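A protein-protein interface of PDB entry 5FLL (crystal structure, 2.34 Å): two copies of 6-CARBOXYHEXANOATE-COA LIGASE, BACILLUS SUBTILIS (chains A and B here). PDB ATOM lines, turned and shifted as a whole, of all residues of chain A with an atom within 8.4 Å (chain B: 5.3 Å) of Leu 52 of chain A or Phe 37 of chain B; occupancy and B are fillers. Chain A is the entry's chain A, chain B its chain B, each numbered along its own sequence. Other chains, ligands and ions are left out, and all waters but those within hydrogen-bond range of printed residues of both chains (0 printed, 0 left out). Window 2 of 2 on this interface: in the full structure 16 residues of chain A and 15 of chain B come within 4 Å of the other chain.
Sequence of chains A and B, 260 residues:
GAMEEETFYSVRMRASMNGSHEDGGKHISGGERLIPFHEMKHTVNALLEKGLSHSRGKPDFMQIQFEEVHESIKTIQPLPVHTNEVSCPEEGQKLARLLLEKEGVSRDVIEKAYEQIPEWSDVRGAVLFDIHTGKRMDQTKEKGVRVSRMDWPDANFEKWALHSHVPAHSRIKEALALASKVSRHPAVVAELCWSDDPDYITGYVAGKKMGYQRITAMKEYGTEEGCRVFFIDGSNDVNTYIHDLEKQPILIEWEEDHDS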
ATOM      1  N   MET A  13     -20.553  26.104  -0.753  1.00  0.00           N
ATOM      2  CA  MET A  13     -20.766  26.199   0.660  1.00  0.00           C
ATOM      3  C   MET A  13     -19.503  26.763   1.304  1.00  0.00           C
ATOM      4  O   MET A  13     -18.381  26.450   0.895  1.00  0.00           O
ATOM      5  CB  MET A  13     -21.062  24.795   1.231  1.00  0.00           C
ATOM      6  CG  MET A  13     -21.240  24.733   2.746  1.00  0.00           C
ATOM      7  SD  MET A  13     -19.689  24.506   3.621  1.00  0.00           S
ATOM      8  CE  MET A  13     -19.262  22.826   3.204  1.00  0.00           C
ATOM      9  N   ALA A  15     -18.275  27.492   5.650  1.00  0.00           N
ATOM     10  CA  ALA A  15     -18.682  27.477   7.031  1.00  0.00           C
ATOM     11  C   ALA A  15     -17.525  27.907   7.936  1.00  0.00           C
ATOM     12  O   ALA A  15     -16.385  27.580   7.679  1.00  0.00           O
ATOM     13  CB  ALA A  15     -19.175  26.079   7.412  1.00  0.00           C
ATOM     14  N   ILE A  28     -13.940  26.600   8.726  1.00  0.00           N
ATOM     15  CA  ILE A  28     -14.174  25.222   9.114  1.00  0.00           C
ATOM     16  C   ILE A  28     -14.206  24.376   7.877  1.00  0.00           C
ATOM     17  O   ILE A  28     -13.464  23.376   7.772  1.00  0.00           O
ATOM     18  CB  ILE A  28     -15.532  25.026   9.837  1.00  0.00           C
ATOM     19  CG1 ILE A  28     -15.560  25.757  11.171  1.00  0.00           C
ATOM     20  CG2 ILE A  28     -15.822  23.537  10.003  1.00  0.00           C
ATOM     21  CD1 ILE A  28     -14.714  25.088  12.236  1.00  0.00           C
ATOM     22  N   SER A  29     -15.064  24.759   6.931  1.00  0.00           N
ATOM     23  CA  SER A  29     -15.253  23.923   5.746  1.00  0.00           C
ATOM     24  C   SER A  29     -15.654  24.730   4.523  1.00  0.00           C
ATOM     25  O   SER A  29     -16.308  25.772   4.632  1.00  0.00           O
ATOM     26  CB  SER A  29     -16.302  22.827   6.004  1.00  0.00           C
ATOM     27  OG  SER A  29     -16.460  22.023   4.824  1.00  0.00           O
ATOM     28  N   ASN A  45     -27.865  19.026   0.796  1.00  0.00           N
ATOM     29  CA  ASN A  45     -27.684  18.224   1.998  1.00  0.00           C
ATOM     30  C   ASN A  45     -26.277  17.658   2.189  1.00  0.00           C
ATOM     31  O   ASN A  45     -25.764  17.581   3.319  1.00  0.00           O
ATOM     32  CB  ASN A  45     -28.689  17.091   2.032  1.00  0.00           C
ATOM     33  CG  ASN A  45     -30.029  17.550   2.550  1.00  0.00           C
ATOM     34  OD1 ASN A  45     -30.229  17.692   3.762  1.00  0.00           O
ATOM     35  ND2 ASN A  45     -30.949  17.819   1.639  1.00  0.00           N
ATOM     36  N   ALA A  46     -25.628  17.275   1.099  1.00  0.00           N
ATOM     37  CA  ALA A  46     -24.269  16.748   1.236  1.00  0.00           C
ATOM     38  C   ALA A  46     -23.354  17.872   1.760  1.00  0.00           C
ATOM     39  O   ALA A  46     -22.617  17.673   2.718  1.00  0.00           O
ATOM     40  CB  ALA A  46     -23.735  16.177  -0.083  1.00  0.00           C
ATOM     41  N   LEU A  47     -23.463  19.053   1.176  1.00  0.00           N
ATOM     42  CA  LEU A  47     -22.643  20.200   1.585  1.00  0.00           C
ATOM     43  C   LEU A  47     -22.967  20.645   3.001  1.00  0.00           C
ATOM     44  O   LEU A  47     -22.072  20.945   3.800  1.00  0.00           O
ATOM     45  CB  LEU A  47     -22.835  21.357   0.615  1.00  0.00           C
ATOM     46  CG  LEU A  47     -22.232  21.180  -0.776  1.00  0.00           C
ATOM     47  CD1 LEU A  47     -22.794  22.192  -1.755  1.00  0.00           C
ATOM     48  CD2 LEU A  47     -20.713  21.305  -0.755  1.00  0.00           C
ATOM     49  N   LEU A  48     -24.254  20.643   3.330  1.00  0.00           N
ATOM     50  CA  LEU A  48     -24.671  20.919   4.685  1.00  0.00           C
ATOM     51  C   LEU A  48     -23.976  19.953   5.653  1.00  0.00           C
ATOM     52  O   LEU A  48     -23.353  20.374   6.630  1.00  0.00           O
ATOM     53  CB  LEU A  48     -26.183  20.797   4.799  1.00  0.00           C
ATOM     54  CG  LEU A  48     -26.771  21.099   6.176  1.00  0.00           C
ATOM     55  CD1 LEU A  48     -26.441  22.525   6.655  1.00  0.00           C
ATOM     56  CD2 LEU A  48     -28.266  20.871   6.143  1.00  0.00           C
ATOM     57  N   GLU A  49     -24.100  18.655   5.392  1.00  0.00           N
ATOM     58  CA  GLU A  49     -23.621  17.636   6.340  1.00  0.00           C
ATOM     59  C   GLU A  49     -22.091  17.747   6.427  1.00  0.00           C
ATOM     60  O   GLU A  49     -21.513  17.634   7.498  1.00  0.00           O
ATOM     61  CB  GLU A  49     -24.058  16.229   5.901  1.00  0.00           C
ATOM     62  CG  GLU A  49     -23.351  15.062   6.589  1.00  0.00           C
ATOM     63  CD  GLU A  49     -23.548  15.027   8.113  1.00  0.00           C
ATOM     64  OE1 GLU A  49     -24.620  15.456   8.605  1.00  0.00           O
ATOM     65  OE2 GLU A  49     -22.617  14.570   8.824  1.00  0.00           O
ATOM     66  N   LYS A  50     -21.457  17.986   5.294  1.00  0.00           N
ATOM     67  CA  LYS A  50     -20.010  18.160   5.248  1.00  0.00           C
ATOM     68  C   LYS A  50     -19.566  19.275   6.168  1.00  0.00           C
ATOM     69  O   LYS A  50     -18.641  19.105   6.946  1.00  0.00           O
ATOM     70  CB  LYS A  50     -19.580  18.459   3.828  1.00  0.00           C
ATOM     71  CG  LYS A  50     -18.135  18.869   3.633  1.00  0.00           C
ATOM     72  CD  LYS A  50     -17.874  19.099   2.152  1.00  0.00           C
ATOM     73  CE  LYS A  50     -16.515  19.737   1.878  1.00  0.00           C
ATOM     74  NZ  LYS A  50     -15.412  18.721   1.866  1.00  0.00           N
ATOM     75  N   GLY A  51     -20.244  20.407   6.098  1.00  0.00           N
ATOM     76  CA  GLY A  51     -19.951  21.507   6.977  1.00  0.00           C
ATOM     77  C   GLY A  51     -20.198  21.239   8.449  1.00  0.00           C
ATOM     78  O   GLY A  51     -19.453  21.749   9.297  1.00  0.00           O
ATOM     79  N   LEU A  52     -21.272  20.487   8.761  1.00  0.00           N
ATOM     80  CA  LEU A  52     -21.735  20.260  10.168  1.00  0.00           C
ATOM     81  C   LEU A  52     -20.918  19.214  10.920  1.00  0.00           C
ATOM     82  O   LEU A  52     -20.905  19.179  12.120  1.00  0.00           O
ATOM     83  CB  LEU A  52     -23.205  19.810  10.206  1.00  0.00           C
ATOM     84  CG  LEU A  52     -24.274  20.810   9.785  1.00  0.00           C
ATOM     85  CD1 LEU A  52     -25.675  20.243   9.934  1.00  0.00           C
ATOM     86  CD2 LEU A  52     -24.147  22.087  10.585  1.00  0.00           C
ATOM     87  N   SER A  53     -20.269  18.320  10.221  1.00  0.00           N
ATOM     88  CA  SER A  53     -19.603  17.230  10.906  1.00  0.00           C
ATOM     89  C   SER A  53     -18.081  17.337  10.717  1.00  0.00           C
ATOM     90  O   SER A  53     -17.397  16.333  10.633  1.00  0.00           O
ATOM     91  CB  SER A  53     -20.112  15.912  10.338  1.00  0.00           C
ATOM     92  OG  SER A  53     -19.836  15.847   8.953  1.00  0.00           O
ATOM     93  N   HIS A  54     -17.555  18.553  10.613  1.00  0.00           N
ATOM     94  CA  HIS A  54     -16.153  18.723  10.298  1.00  0.00           C
ATOM     95  C   HIS A  54     -15.272  18.564  11.530  1.00  0.00           C
ATOM     96  O   HIS A  54     -15.622  19.023  12.613  1.00  0.00           O
ATOM     97  CB  HIS A  54     -15.897  20.083   9.637  1.00  0.00           C
ATOM     98  CG  HIS A  54     -14.669  20.110   8.790  1.00  0.00           C
ATOM     99  ND1 HIS A  54     -13.400  20.150   9.323  1.00  0.00           N
ATOM    100  CD2 HIS A  54     -14.512  20.069   7.443  1.00  0.00           C
ATOM    101  CE1 HIS A  54     -12.515  20.149   8.339  1.00  0.00           C
ATOM    102  NE2 HIS A  54     -13.165  20.107   7.188  1.00  0.00           N
ATOM    103  N   SER A  55     -14.113  17.941  11.338  1.00  0.00           N
ATOM    104  CA  SER A  55     -13.134  17.712  12.418  1.00  0.00           C
ATOM    105  C   SER A  55     -12.511  18.987  12.984  1.00  0.00           C
ATOM    106  O   SER A  55     -12.089  18.995  14.126  1.00  0.00           O
ATOM    107  CB  SER A  55     -11.998  16.782  11.944  1.00  0.00           C
ATOM    108  OG  SER A  55     -11.297  17.324  10.819  1.00  0.00           O
ATOM    109  N   GLY A  57     -14.327  21.491  13.691  1.00  0.00           N
ATOM    110  CA  GLY A  57     -15.315  22.001  14.633  1.00  0.00           C
ATOM    111  C   GLY A  57     -16.704  22.259  14.040  1.00  0.00           C
ATOM    112  O   GLY A  57     -16.935  22.155  12.819  1.00  0.00           O
ATOM    113  N   LYS A  58     -17.607  22.614  14.932  1.00  0.00           N
ATOM    114  CA  LYS A  58     -18.962  22.952  14.620  1.00  0.00           C
ATOM    115  C   LYS A  58     -19.067  24.418  14.216  1.00  0.00           C
ATOM    116  O   LYS A  58     -18.695  25.301  14.973  1.00  0.00           O
ATOM    117  CB  LYS A  58     -19.826  22.732  15.864  1.00  0.00           C
ATOM    118  CG  LYS A  58     -21.195  23.377  15.766  1.00  0.00           C
ATOM    119  CD  LYS A  58     -21.804  23.610  17.139  1.00  0.00           C
ATOM    120  CE  LYS A  58     -23.119  24.365  17.031  1.00  0.00           C
ATOM    121  NZ  LYS A  58     -23.844  24.375  18.336  1.00  0.00           N
ATOM    122  N   PRO A  59     -19.604  24.690  13.032  1.00  0.00           N
ATOM    123  CA  PRO A  59     -19.724  26.083  12.614  1.00  0.00           C
ATOM    124  C   PRO A  59     -20.855  26.798  13.343  1.00  0.00           C
ATOM    125  O   PRO A  59     -21.801  26.170  13.753  1.00  0.00           O
ATOM    126  CB  PRO A  59     -20.011  25.983  11.117  1.00  0.00           C
ATOM    127  CG  PRO A  59     -20.554  24.616  10.914  1.00  0.00           C
ATOM    128  CD  PRO A  59     -19.933  23.747  11.961  1.00  0.00           C
ATOM    129  N   ASP A  60     -20.722  28.107  13.521  1.00  0.00           N
ATOM    130  CA  ASP A  60     -21.832  28.963  13.906  1.00  0.00           C
ATOM    131  C   ASP A  60     -22.259  29.875  12.740  1.00  0.00           C
ATOM    132  O   ASP A  60     -23.106  30.753  12.899  1.00  0.00           O
ATOM    133  CB  ASP A  60     -21.449  29.808  15.132  1.00  0.00           C
ATOM    134  CG  ASP A  60     -20.219  30.635  14.893  1.00  0.00           C
ATOM    135  OD1 ASP A  60     -20.037  31.147  13.767  1.00  0.00           O
ATOM    136  OD2 ASP A  60     -19.415  30.763  15.828  1.00  0.00           O
ATOM    137  N   PHE A  61     -21.637  29.670  11.581  1.00  0.00           N
ATOM    138  CA  PHE A  61     -21.993  30.383  10.372  1.00  0.00           C
ATOM    139  C   PHE A  61     -21.848  29.466   9.177  1.00  0.00           C
ATOM    140  O   PHE A  61     -20.843  28.781   9.039  1.00  0.00           O
ATOM    141  CB  PHE A  61     -21.093  31.618  10.189  1.00  0.00           C
ATOM    142  CG  PHE A  61     -21.333  32.367   8.886  1.00  0.00           C
ATOM    143  CD1 PHE A  61     -20.656  32.008   7.722  1.00  0.00           C
ATOM    144  CD2 PHE A  61     -22.204  33.452   8.844  1.00  0.00           C
ATOM    145  CE1 PHE A  61     -20.867  32.682   6.549  1.00  0.00           C
ATOM    146  CE2 PHE A  61     -22.417  34.143   7.655  1.00  0.00           C
ATOM    147  CZ  PHE A  61     -21.753  33.742   6.506  1.00  0.00           C
ATOM    148  N   MET A  62     -22.816  29.496   8.271  1.00  0.00           N
ATOM    149  CA  MET A  62     -22.688  28.764   7.005  1.00  0.00           C
ATOM    150  C   MET A  62     -23.525  29.404   5.909  1.00  0.00           C
ATOM    151  O   MET A  62     -24.578  29.947   6.165  1.00  0.00           O
ATOM    152  CB  MET A  62     -23.100  27.305   7.187  1.00  0.00           C
ATOM    153  CG  MET A  62     -23.072  26.465   5.904  1.00  0.00           C
ATOM    154  SD  MET A  62     -23.473  24.691   6.091  1.00  0.00           S
ATOM    155  CE  MET A  62     -22.668  24.328   7.672  1.00  0.00           C
ATOM    156  N   ILE A  64     -24.831  28.472   1.858  1.00  0.00           N
ATOM    157  CA  ILE A  64     -24.904  27.555   0.741  1.00  0.00           C
ATOM    158  C   ILE A  64     -25.611  28.292  -0.362  1.00  0.00           C
ATOM    159  O   ILE A  64     -26.605  28.971  -0.132  1.00  0.00           O
ATOM    160  CB  ILE A  64     -25.741  26.316   1.076  1.00  0.00           C
ATOM    161  CG1 ILE A  64     -25.102  25.563   2.247  1.00  0.00           C
ATOM    162  CG2 ILE A  64     -25.853  25.417  -0.130  1.00  0.00           C
ATOM    163  CD1 ILE A  64     -25.841  24.286   2.680  1.00  0.00           C
ATOM    164  N   THR B   7     -29.128  27.927  22.580  1.00  0.00           N
ATOM    165  CA  THR B   7     -28.645  28.811  21.549  1.00  0.00           C
ATOM    166  C   THR B   7     -29.541  28.726  20.321  1.00  0.00           C
ATOM    167  O   THR B   7     -29.842  27.627  19.839  1.00  0.00           O
ATOM    168  CB  THR B   7     -27.186  28.459  21.220  1.00  0.00           C
ATOM    169  OG1 THR B   7     -26.376  28.729  22.376  1.00  0.00           O
ATOM    170  CG2 THR B   7     -26.688  29.273  20.083  1.00  0.00           C
ATOM    171  N   TYR B   9     -30.495  30.063  16.206  1.00  0.00           N
ATOM    172  CA  TYR B   9     -29.877  30.408  14.919  1.00  0.00           C
ATOM    173  C   TYR B   9     -30.871  31.054  13.986  1.00  0.00           C
ATOM    174  O   TYR B   9     -32.018  30.621  13.872  1.00  0.00           O
ATOM    175  CB  TYR B   9     -29.282  29.165  14.239  1.00  0.00           C
ATOM    176  CG  TYR B   9     -28.151  28.584  15.042  1.00  0.00           C
ATOM    177  CD1 TYR B   9     -28.406  27.888  16.210  1.00  0.00           C
ATOM    178  CD2 TYR B   9     -26.829  28.785  14.672  1.00  0.00           C
ATOM    179  CE1 TYR B   9     -27.369  27.395  16.993  1.00  0.00           C
ATOM    180  CE2 TYR B   9     -25.782  28.289  15.439  1.00  0.00           C
ATOM    181  CZ  TYR B   9     -26.064  27.603  16.598  1.00  0.00           C
ATOM    182  OH  TYR B   9     -25.037  27.108  17.355  1.00  0.00           O
ATOM    183  N   ILE B  35     -34.374  29.294  15.191  1.00  0.00           N
ATOM    184  CA  ILE B  35     -34.444  27.896  15.631  1.00  0.00           C
ATOM    185  C   ILE B  35     -33.288  27.438  16.486  1.00  0.00           C
ATOM    186  O   ILE B  35     -32.172  27.934  16.350  1.00  0.00           O
ATOM    187  CB  ILE B  35     -34.424  26.941  14.429  1.00  0.00           C
ATOM    188  CG1 ILE B  35     -33.150  27.151  13.628  1.00  0.00           C
ATOM    189  CG2 ILE B  35     -35.642  27.163  13.552  1.00  0.00           C
ATOM    190  CD1 ILE B  35     -32.775  25.982  12.746  1.00  0.00           C
ATOM    191  N   PRO B  36     -33.525  26.408  17.299  1.00  0.00           N
ATOM    192  CA  PRO B  36     -32.423  25.746  17.940  1.00  0.00           C
ATOM    193  C   PRO B  36     -31.611  24.961  16.931  1.00  0.00           C
ATOM    194  O   PRO B  36     -32.114  24.614  15.865  1.00  0.00           O
ATOM    195  CB  PRO B  36     -33.101  24.825  18.951  1.00  0.00           C
ATOM    196  CG  PRO B  36     -34.481  24.617  18.464  1.00  0.00           C
ATOM    197  CD  PRO B  36     -34.832  25.827  17.668  1.00  0.00           C
ATOM    198  N   PHE B  37     -30.368  24.679  17.268  1.00  0.00           N
ATOM    199  CA  PHE B  37     -29.444  24.064  16.329  1.00  0.00           C
ATOM    200  C   PHE B  37     -29.933  22.719  15.789  1.00  0.00           C
ATOM    201  O   PHE B  37     -29.693  22.392  14.630  1.00  0.00           O
ATOM    202  CB  PHE B  37     -28.076  23.888  16.972  1.00  0.00           C
ATOM    203  CG  PHE B  37     -26.984  23.554  15.991  1.00  0.00           C
ATOM    204  CD1 PHE B  37     -26.465  24.530  15.148  1.00  0.00           C
ATOM    205  CD2 PHE B  37     -26.466  22.270  15.918  1.00  0.00           C
ATOM    206  CE1 PHE B  37     -25.443  24.233  14.257  1.00  0.00           C
ATOM    207  CE2 PHE B  37     -25.454  21.959  15.032  1.00  0.00           C
ATOM    208  CZ  PHE B  37     -24.933  22.946  14.205  1.00  0.00           C
ATOM    209  N   HIS B  38     -30.620  21.945  16.624  1.00  0.00           N
ATOM    210  CA  HIS B  38     -30.992  20.565  16.245  1.00  0.00           C
ATOM    211  C   HIS B  38     -32.082  20.545  15.175  1.00  0.00           C
ATOM    212  O   HIS B  38     -32.288  19.531  14.525  1.00  0.00           O
ATOM    213  CB  HIS B  38     -31.411  19.744  17.467  1.00  0.00           C
ATOM    214  CG  HIS B  38     -32.673  20.210  18.105  1.00  0.00           C
ATOM    215  ND1 HIS B  38     -32.684  21.012  19.227  1.00  0.00           N
ATOM    216  CD2 HIS B  38     -33.973  19.984  17.787  1.00  0.00           C
ATOM    217  CE1 HIS B  38     -33.937  21.247  19.586  1.00  0.00           C
ATOM    218  NE2 HIS B  38     -34.738  20.646  18.722  1.00  0.00           N
ATOM    219  N   GLU B  39     -32.767  21.668  14.965  1.00  0.00           N
ATOM    220  CA  GLU B  39     -33.710  21.752  13.846  1.00  0.00           C
ATOM    221  C   GLU B  39     -33.051  22.209  12.535  1.00  0.00           C
ATOM    222  O   GLU B  39     -33.733  22.448  11.559  1.00  0.00           O
ATOM    223  CB  GLU B  39     -34.907  22.636  14.198  1.00  0.00           C
ATOM    224  CG  GLU B  39     -35.861  21.979  15.177  1.00  0.00           C
ATOM    225  CD  GLU B  39     -36.838  22.963  15.805  1.00  0.00           C
ATOM    226  OE1 GLU B  39     -37.183  23.993  15.186  1.00  0.00           O
ATOM    227  OE2 GLU B  39     -37.267  22.720  16.946  1.00  0.00           O
ATOM    228  N   MET B  40     -31.730  22.264  12.486  1.00  0.00           N
ATOM    229  CA  MET B  40     -31.072  22.919  11.377  1.00  0.00           C
ATOM    230  C   MET B  40     -31.365  22.210  10.045  1.00  0.00           C
ATOM    231  O   MET B  40     -31.734  22.847   9.066  1.00  0.00           O
ATOM    232  CB  MET B  40     -29.580  23.012  11.618  1.00  0.00           C
ATOM    233  CG  MET B  40     -28.852  23.888  10.580  1.00  0.00           C
ATOM    234  SD  MET B  40     -29.485  25.572  10.372  1.00  0.00           S
ATOM    235  CE  MET B  40     -28.899  26.263  11.911  1.00  0.00           C
ATOM    236  N   LYS B  41     -31.225  20.895  10.015  1.00  0.00           N
ATOM    237  CA  LYS B  41     -31.430  20.134   8.795  1.00  0.00           C
ATOM    238  C   LYS B  41     -32.851  20.238   8.284  1.00  0.00           C
ATOM    239  O   LYS B  41     -33.053  20.458   7.075  1.00  0.00           O
ATOM    240  CB  LYS B  41     -31.066  18.667   8.973  1.00  0.00           C
ATOM    241  CG  LYS B  41     -29.590  18.431   8.809  1.00  0.00           C
ATOM    242  CD  LYS B  41     -29.248  16.964   8.933  1.00  0.00           C
ATOM    243  CE  LYS B  41     -27.744  16.752   9.047  1.00  0.00           C
ATOM    244  NZ  LYS B  41     -27.269  15.724   8.082  1.00  0.00           N
ATOM    245  N   PHE B  66     -27.075  30.344   7.597  1.00  0.00           N
ATOM    246  CA  PHE B  66     -27.367  30.414   9.019  1.00  0.00           C
ATOM    247  C   PHE B  66     -26.266  31.101   9.799  1.00  0.00           C
ATOM    248  O   PHE B  66     -25.124  31.133   9.361  1.00  0.00           O
ATOM    249  CB  PHE B  66     -27.791  29.067   9.629  1.00  0.00           C
ATOM    250  CG  PHE B  66     -26.682  28.104   9.854  1.00  0.00           C
ATOM    251  CD1 PHE B  66     -25.761  28.308  10.859  1.00  0.00           C
ATOM    252  CD2 PHE B  66     -26.627  26.928   9.126  1.00  0.00           C
ATOM    253  CE1 PHE B  66     -24.757  27.378  11.109  1.00  0.00           C
ATOM    254  CE2 PHE B  66     -25.622  25.988   9.355  1.00  0.00           C
ATOM    255  CZ  PHE B  66     -24.678  26.214  10.351  1.00  0.00           C
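The backbone carbonyl oxygen of Met 62 of chain A is in hydrogen-bond range of the backbone NH of Phe 66 of chain B (2.9 Å). OE1 of Glu 49 of chain A is in salt-bridge range of NZ of Lys 41 of chain B (2.7 Å). NZ of Lys 58 of chain A sits at hydrogen-bond distance from OH of Tyr 9 of chain B (3.1 Å).
The backbone carbonyl oxygen (O) of Glu 49 of chain A sits at hydrogen-bond distance from the side-chain hydroxyl (OG) of Ser 53 of chain A (2.9 Å). N of Tyr 9 of chain B is in hydrogen-bond range of O of Ile 35 of chain B (2.7 Å).
Leu 48 of chain A touches Lys 41 of chain B (CD2 to CG, 3.8 Å). CD2 of Leu 52 of chain A touches CZ of Phe 37 of chain B, 3.8 Å away. CE1 of Phe 37 of chain B touches CE of Lys 58 of chain A, at 3.6 Å. C of Asp 60 of chain A touches CE1 of Phe 66 of chain B (3.9 Å). O of Phe 66 of chain B touches CA of Phe 61 of chain A, at 3.4 Å.
Ala 15 of chain A touches none of the printed residues of chain B. Ala 46 of chain A touches none of the printed residues of chain B. Printed residues of chain B within 4 Å of Leu 48 of chain A: Lys 41. Leu 52 of chain A touches one residue of chain B. Of the printed residues of chain B, Lys 58 of chain A touches Tyr 9 and Phe 37. Of the printed residues of chain B, Met 62 of chain A touches Phe 66 (2.9 Å). Phe 37 of chain B touches just these residues of chain A: Leu 52 (3.8 Å) and Lys 58 (3.6 Å). Of the printed residues of chain A, Phe 66 of chain B touches Asp 60, Phe 61 and Met 62. The nearest residue of chain A that does not touch Phe 37 of chain B is Pro 59 of chain A (4.2 Å).
Of the 22 printed residues of chain A, 7 touch a printed residue of chain B. Hydrophobic or aromatic side chains of chain A within 4 Å of the printed part of chain B: Leu 48, Leu 52, Phe 61 and Met 62. Of the 10 printed residues of chain B, 4 touch a printed residue of chain A. Printed residues of chain B that touch a printed residue of chain A: Tyr 9, Phe 37, Lys 41 and Phe 66. Among the printed residues, 8 pairs touch across the chains.
No position is printed for both chains. Of the 8 pairs that touch across the chains among the printed residues, none has its exchanged pair printed and touching as well.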
